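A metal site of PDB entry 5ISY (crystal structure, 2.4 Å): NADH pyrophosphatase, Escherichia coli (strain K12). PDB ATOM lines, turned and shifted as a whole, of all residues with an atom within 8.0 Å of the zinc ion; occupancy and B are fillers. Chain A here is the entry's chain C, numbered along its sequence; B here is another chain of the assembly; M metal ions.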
ATOM      1  N   TYR A  99      20.373 -22.954   0.651  1.00  0.00           N
ATOM      2  CA  TYR A  99      21.753 -23.168   1.037  1.00  0.00           C
ATOM      3  C   TYR A  99      21.874 -23.482   2.521  1.00  0.00           C
ATOM      4  O   TYR A  99      21.069 -23.008   3.341  1.00  0.00           O
ATOM      5  CB  TYR A  99      22.598 -21.939   0.715  1.00  0.00           C
ATOM      6  CG  TYR A  99      22.566 -21.598  -0.741  1.00  0.00           C
ATOM      7  CD1 TYR A  99      21.606 -20.733  -1.254  1.00  0.00           C
ATOM      8  CD2 TYR A  99      23.498 -22.146  -1.615  1.00  0.00           C
ATOM      9  CE1 TYR A  99      21.575 -20.424  -2.572  1.00  0.00           C
ATOM     10  CE2 TYR A  99      23.474 -21.839  -2.953  1.00  0.00           C
ATOM     11  CZ  TYR A  99      22.502 -20.983  -3.433  1.00  0.00           C
ATOM     12  OH  TYR A  99      22.454 -20.675  -4.765  1.00  0.00           O
ATOM     13  N   CYS A 100      22.911 -24.229   2.882  1.00  0.00           N
ATOM     14  CA  CYS A 100      23.177 -24.553   4.278  1.00  0.00           C
ATOM     15  C   CYS A 100      23.882 -23.386   4.963  1.00  0.00           C
ATOM     16  O   CYS A 100      24.960 -22.976   4.539  1.00  0.00           O
ATOM     17  CB  CYS A 100      24.017 -25.833   4.384  1.00  0.00           C
ATOM     18  SG  CYS A 100      24.569 -26.199   6.079  1.00  0.00           S
ATOM     19  N   GLY A 101      23.286 -22.871   6.039  1.00  0.00           N
ATOM     20  CA  GLY A 101      23.902 -21.762   6.748  1.00  0.00           C
ATOM     21  C   GLY A 101      25.216 -22.111   7.428  1.00  0.00           C
ATOM     22  O   GLY A 101      25.999 -21.207   7.733  1.00  0.00           O
ATOM     23  N   TYR A 102      25.461 -23.395   7.695  1.00  0.00           N
ATOM     24  CA  TYR A 102      26.720 -23.797   8.315  1.00  0.00           C
ATOM     25  C   TYR A 102      27.861 -23.783   7.308  1.00  0.00           C
ATOM     26  O   TYR A 102      28.877 -23.110   7.514  1.00  0.00           O
ATOM     27  CB  TYR A 102      26.614 -25.195   8.945  1.00  0.00           C
ATOM     28  CG  TYR A 102      25.685 -25.289  10.158  1.00  0.00           C
ATOM     29  CD1 TYR A 102      26.150 -25.074  11.460  1.00  0.00           C
ATOM     30  CD2 TYR A 102      24.327 -25.604   9.991  1.00  0.00           C
ATOM     31  CE1 TYR A 102      25.286 -25.176  12.568  1.00  0.00           C
ATOM     32  CE2 TYR A 102      23.461 -25.724  11.075  1.00  0.00           C
ATOM     33  CZ  TYR A 102      23.943 -25.506  12.364  1.00  0.00           C
ATOM     34  OH  TYR A 102      23.064 -25.604  13.428  1.00  0.00           O
ATOM     35  N   CYS A 103      27.690 -24.502   6.196  1.00  0.00           N
ATOM     36  CA  CYS A 103      28.789 -24.803   5.289  1.00  0.00           C
ATOM     37  C   CYS A 103      28.623 -24.224   3.894  1.00  0.00           C
ATOM     38  O   CYS A 103      29.616 -24.156   3.151  1.00  0.00           O
ATOM     39  CB  CYS A 103      28.968 -26.317   5.174  1.00  0.00           C
ATOM     40  SG  CYS A 103      27.741 -27.003   4.072  1.00  0.00           S
ATOM     41  N   GLY A 104      27.419 -23.808   3.512  1.00  0.00           N
ATOM     42  CA  GLY A 104      27.209 -23.068   2.286  1.00  0.00           C
ATOM     43  C   GLY A 104      26.805 -23.897   1.086  1.00  0.00           C
ATOM     44  O   GLY A 104      26.486 -23.320   0.041  1.00  0.00           O
ATOM     45  N   HIS A 105      26.812 -25.222   1.195  1.00  0.00           N
ATOM     46  CA  HIS A 105      26.363 -26.064   0.098  1.00  0.00           C
ATOM     47  C   HIS A 105      24.841 -26.096   0.032  1.00  0.00           C
ATOM     48  O   HIS A 105      24.128 -25.726   0.970  1.00  0.00           O
ATOM     49  CB  HIS A 105      26.930 -27.476   0.254  1.00  0.00           C
ATOM     50  CG  HIS A 105      28.398 -27.541   0.013  1.00  0.00           C
ATOM     51  ND1 HIS A 105      29.323 -27.100   0.943  1.00  0.00           N
ATOM     52  CD2 HIS A 105      29.115 -27.939  -1.064  1.00  0.00           C
ATOM     53  CE1 HIS A 105      30.540 -27.240   0.446  1.00  0.00           C
ATOM     54  NE2 HIS A 105      30.446 -27.755  -0.765  1.00  0.00           N
ATOM     55  N   GLU A 106      24.334 -26.529  -1.122  1.00  0.00           N
ATOM     56  CA  GLU A 106      22.897 -26.647  -1.317  1.00  0.00           C
ATOM     57  C   GLU A 106      22.337 -27.809  -0.497  1.00  0.00           C
ATOM     58  O   GLU A 106      22.966 -28.857  -0.384  1.00  0.00           O
ATOM     59  CB  GLU A 106      22.575 -26.843  -2.804  1.00  0.00           C
ATOM     60  CG  GLU A 106      22.768 -25.570  -3.617  1.00  0.00           C
ATOM     61  CD  GLU A 106      22.617 -25.794  -5.093  1.00  0.00           C
ATOM     62  OE1 GLU A 106      21.480 -26.029  -5.548  1.00  0.00           O
ATOM     63  OE2 GLU A 106      23.647 -25.764  -5.804  1.00  0.00           O
ATOM     64  N   MET A 107      21.175 -27.574   0.085  1.00  0.00           N
ATOM     65  CA  MET A 107      20.450 -28.579   0.854  1.00  0.00           C
ATOM     66  C   MET A 107      19.386 -29.215  -0.034  1.00  0.00           C
ATOM     67  O   MET A 107      19.133 -28.779  -1.152  1.00  0.00           O
ATOM     68  CB  MET A 107      19.787 -27.959   2.098  1.00  0.00           C
ATOM     69  CG  MET A 107      20.688 -27.091   2.967  1.00  0.00           C
ATOM     70  SD  MET A 107      19.996 -26.557   4.576  1.00  0.00           S
ATOM     71  CE  MET A 107      20.358 -28.031   5.515  1.00  0.00           C
ATOM     72  N   LEU A 117      18.028 -30.796   4.816  1.00  0.00           N
ATOM     73  CA  LEU A 117      19.187 -31.598   5.168  1.00  0.00           C
ATOM     74  C   LEU A 117      20.391 -31.172   4.337  1.00  0.00           C
ATOM     75  O   LEU A 117      20.243 -30.821   3.163  1.00  0.00           O
ATOM     76  CB  LEU A 117      18.895 -33.096   4.928  1.00  0.00           C
ATOM     77  CG  LEU A 117      18.148 -34.005   5.909  1.00  0.00           C
ATOM     78  CD1 LEU A 117      17.201 -33.281   6.819  1.00  0.00           C
ATOM     79  CD2 LEU A 117      17.419 -35.108   5.124  1.00  0.00           C
ATOM     80  N   CYS A 118      21.583 -31.211   4.937  1.00  0.00           N
ATOM     81  CA  CYS A 118      22.844 -30.953   4.244  1.00  0.00           C
ATOM     82  C   CYS A 118      23.609 -32.252   4.066  1.00  0.00           C
ATOM     83  O   CYS A 118      24.089 -32.841   5.052  1.00  0.00           O
ATOM     84  CB  CYS A 118      23.707 -29.941   4.987  1.00  0.00           C
ATOM     85  SG  CYS A 118      25.078 -29.350   3.970  1.00  0.00           S
ATOM     86  N   SER A 119      23.753 -32.699   2.823  1.00  0.00           N
ATOM     87  CA  SER A 119      24.628 -33.835   2.535  1.00  0.00           C
ATOM     88  C   SER A 119      26.062 -33.544   2.973  1.00  0.00           C
ATOM     89  O   SER A 119      26.738 -34.399   3.548  1.00  0.00           O
ATOM     90  CB  SER A 119      24.577 -34.170   1.049  1.00  0.00           C
ATOM     91  OG  SER A 119      25.204 -33.168   0.275  1.00  0.00           O
ATOM     92  N   HIS A 120      26.538 -32.317   2.722  1.00  0.00           N
ATOM     93  CA  HIS A 120      27.975 -32.061   2.842  1.00  0.00           C
ATOM     94  C   HIS A 120      28.442 -31.997   4.296  1.00  0.00           C
ATOM     95  O   HIS A 120      29.500 -32.542   4.619  1.00  0.00           O
ATOM     96  CB  HIS A 120      28.343 -30.770   2.109  1.00  0.00           C
ATOM     97  CG  HIS A 120      29.799 -30.446   2.167  1.00  0.00           C
ATOM     98  ND1 HIS A 120      30.346 -29.641   3.156  1.00  0.00           N
ATOM     99  CD2 HIS A 120      30.837 -30.822   1.369  1.00  0.00           C
ATOM    100  CE1 HIS A 120      31.653 -29.531   2.959  1.00  0.00           C
ATOM    101  NE2 HIS A 120      31.973 -30.241   1.897  1.00  0.00           N
ATOM    102  N   CYS A 121      27.694 -31.337   5.199  1.00  0.00           N
ATOM    103  CA  CYS A 121      28.140 -31.217   6.588  1.00  0.00           C
ATOM    104  C   CYS A 121      27.264 -31.924   7.618  1.00  0.00           C
ATOM    105  O   CYS A 121      27.642 -31.977   8.796  1.00  0.00           O
ATOM    106  CB  CYS A 121      28.298 -29.738   6.991  1.00  0.00           C
ATOM    107  SG  CYS A 121      26.731 -28.850   7.340  1.00  0.00           S
ATOM    108  N   ARG A 122      26.096 -32.438   7.219  1.00  0.00           N
ATOM    109  CA  ARG A 122      25.236 -33.294   8.037  1.00  0.00           C
ATOM    110  C   ARG A 122      24.503 -32.546   9.145  1.00  0.00           C
ATOM    111  O   ARG A 122      24.013 -33.176  10.079  1.00  0.00           O
ATOM    112  CB  ARG A 122      26.023 -34.477   8.617  1.00  0.00           C
ATOM    113  CG  ARG A 122      26.656 -35.320   7.508  1.00  0.00           C
ATOM    114  CD  ARG A 122      26.390 -36.790   7.672  1.00  0.00           C
ATOM    115  NE  ARG A 122      27.289 -37.425   8.648  1.00  0.00           N
ATOM    116  CZ  ARG A 122      28.279 -38.263   8.331  1.00  0.00           C
ATOM    117  NH1 ARG A 122      29.028 -38.789   9.286  1.00  0.00           N
ATOM    118  NH2 ARG A 122      28.509 -38.569   7.060  1.00  0.00           N
ATOM    119  N   GLU A 123      24.379 -31.227   9.045  1.00  0.00           N
ATOM    120  CA  GLU A 123      23.462 -30.475   9.888  1.00  0.00           C
ATOM    121  C   GLU A 123      22.096 -30.396   9.200  1.00  0.00           C
ATOM    122  O   GLU A 123      21.961 -30.589   7.993  1.00  0.00           O
ATOM    123  CB  GLU A 123      23.988 -29.051  10.142  1.00  0.00           C
ATOM    124  CG  GLU A 123      25.359 -28.974  10.779  1.00  0.00           C
ATOM    125  CD  GLU A 123      25.337 -29.211  12.274  1.00  0.00           C
ATOM    126  OE1 GLU A 123      24.222 -29.243  12.852  1.00  0.00           O
ATOM    127  OE2 GLU A 123      26.426 -29.365  12.877  1.00  0.00           O
ATOM    128  N   ARG A 124      21.069 -30.059   9.994  1.00  0.00           N
ATOM    129  CA  ARG A 124      19.715 -29.951   9.446  1.00  0.00           C
ATOM    130  C   ARG A 124      18.996 -28.769  10.081  1.00  0.00           C
ATOM    131  O   ARG A 124      19.444 -28.187  11.073  1.00  0.00           O
ATOM    132  CB  ARG A 124      18.921 -31.240   9.669  1.00  0.00           C
ATOM    133  CG  ARG A 124      18.720 -31.567  11.131  1.00  0.00           C
ATOM    134  CD  ARG A 124      17.559 -32.510  11.334  1.00  0.00           C
ATOM    135  NE  ARG A 124      17.959 -33.868  11.669  1.00  0.00           N
ATOM    136  CZ  ARG A 124      18.086 -34.333  12.906  1.00  0.00           C
ATOM    137  NH1 ARG A 124      18.442 -35.589  13.109  1.00  0.00           N
ATOM    138  NH2 ARG A 124      17.852 -33.541  13.947  1.00  0.00           N
ATOM    139  N   TYR A 125      17.850 -28.413   9.495  1.00  0.00           N
ATOM    140  CA  TYR A 125      16.988 -27.369  10.036  1.00  0.00           C
ATOM    141  C   TYR A 125      15.533 -27.838  10.016  1.00  0.00           C
ATOM    142  O   TYR A 125      15.112 -28.552   9.109  1.00  0.00           O
ATOM    143  CB  TYR A 125      17.051 -26.069   9.220  1.00  0.00           C
ATOM    144  CG  TYR A 125      18.390 -25.380   9.128  1.00  0.00           C
ATOM    145  CD1 TYR A 125      19.352 -25.828   8.246  1.00  0.00           C
ATOM    146  CD2 TYR A 125      18.664 -24.250   9.883  1.00  0.00           C
ATOM    147  CE1 TYR A 125      20.568 -25.185   8.143  1.00  0.00           C
ATOM    148  CE2 TYR A 125      19.880 -23.594   9.774  1.00  0.00           C
ATOM    149  CZ  TYR A 125      20.821 -24.066   8.896  1.00  0.00           C
ATOM    150  OH  TYR A 125      22.025 -23.416   8.793  1.00  0.00           O
ATOM    151  N   TYR B  99      26.424 -18.638   6.424  1.00  0.00           N
ATOM    152  CA  TYR B  99      25.926 -18.399   5.072  1.00  0.00           C
ATOM    153  C   TYR B  99      24.420 -18.126   5.066  1.00  0.00           C
ATOM    154  O   TYR B  99      23.668 -18.640   5.890  1.00  0.00           O
ATOM    155  CB  TYR B  99      26.237 -19.601   4.160  1.00  0.00           C
ATOM    156  CG  TYR B  99      27.726 -19.870   4.051  1.00  0.00           C
ATOM    157  CD1 TYR B  99      28.486 -19.245   3.070  1.00  0.00           C
ATOM    158  CD2 TYR B  99      28.352 -20.744   4.935  1.00  0.00           C
ATOM    159  CE1 TYR B  99      29.835 -19.473   2.975  1.00  0.00           C
ATOM    160  CE2 TYR B  99      29.714 -20.981   4.853  1.00  0.00           C
ATOM    161  CZ  TYR B  99      30.451 -20.353   3.865  1.00  0.00           C
ATOM    162  OH  TYR B  99      31.789 -20.586   3.761  1.00  0.00           O
HETATM  163 ZN    ZN M   1      26.083 -27.915   5.443  1.00  0.00          ZN
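Four residues have an atom within 4 Å of the zinc ion: Cys 100, Cys 103, Cys 118 and Cys 121.
Along chain A the residues within 4 Å of the zinc ion span positions 100 to 121.
The side-chain sulfur (SG) of Cys 121 sits close to the backbone NH (N) of Glu 123, 3.8 Å away.
SG of Cys 118 lies close to N of His 120, at 3.5 Å.
N of Cys 118 sits at hydrogen-bond distance from O of Glu 123 (3.1 Å).
SG of Cys 103 sits close to ND1 of His 105 (3.5 Å).
SG of Cys 100 lies close to N of Tyr 102.
The backbone NH of Cys 100 sits at hydrogen-bond distance from the backbone carbonyl oxygen of His 105 (2.7 Å).
SG of Cys 121 binds the zinc ion.
The side-chain sulfur (SG) of Cys 118 binds the zinc ion, 2.3 Å away.
SG of Cys 103 binds the zinc ion.
SG of Cys 100 binds the zinc ion (2.4 Å).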
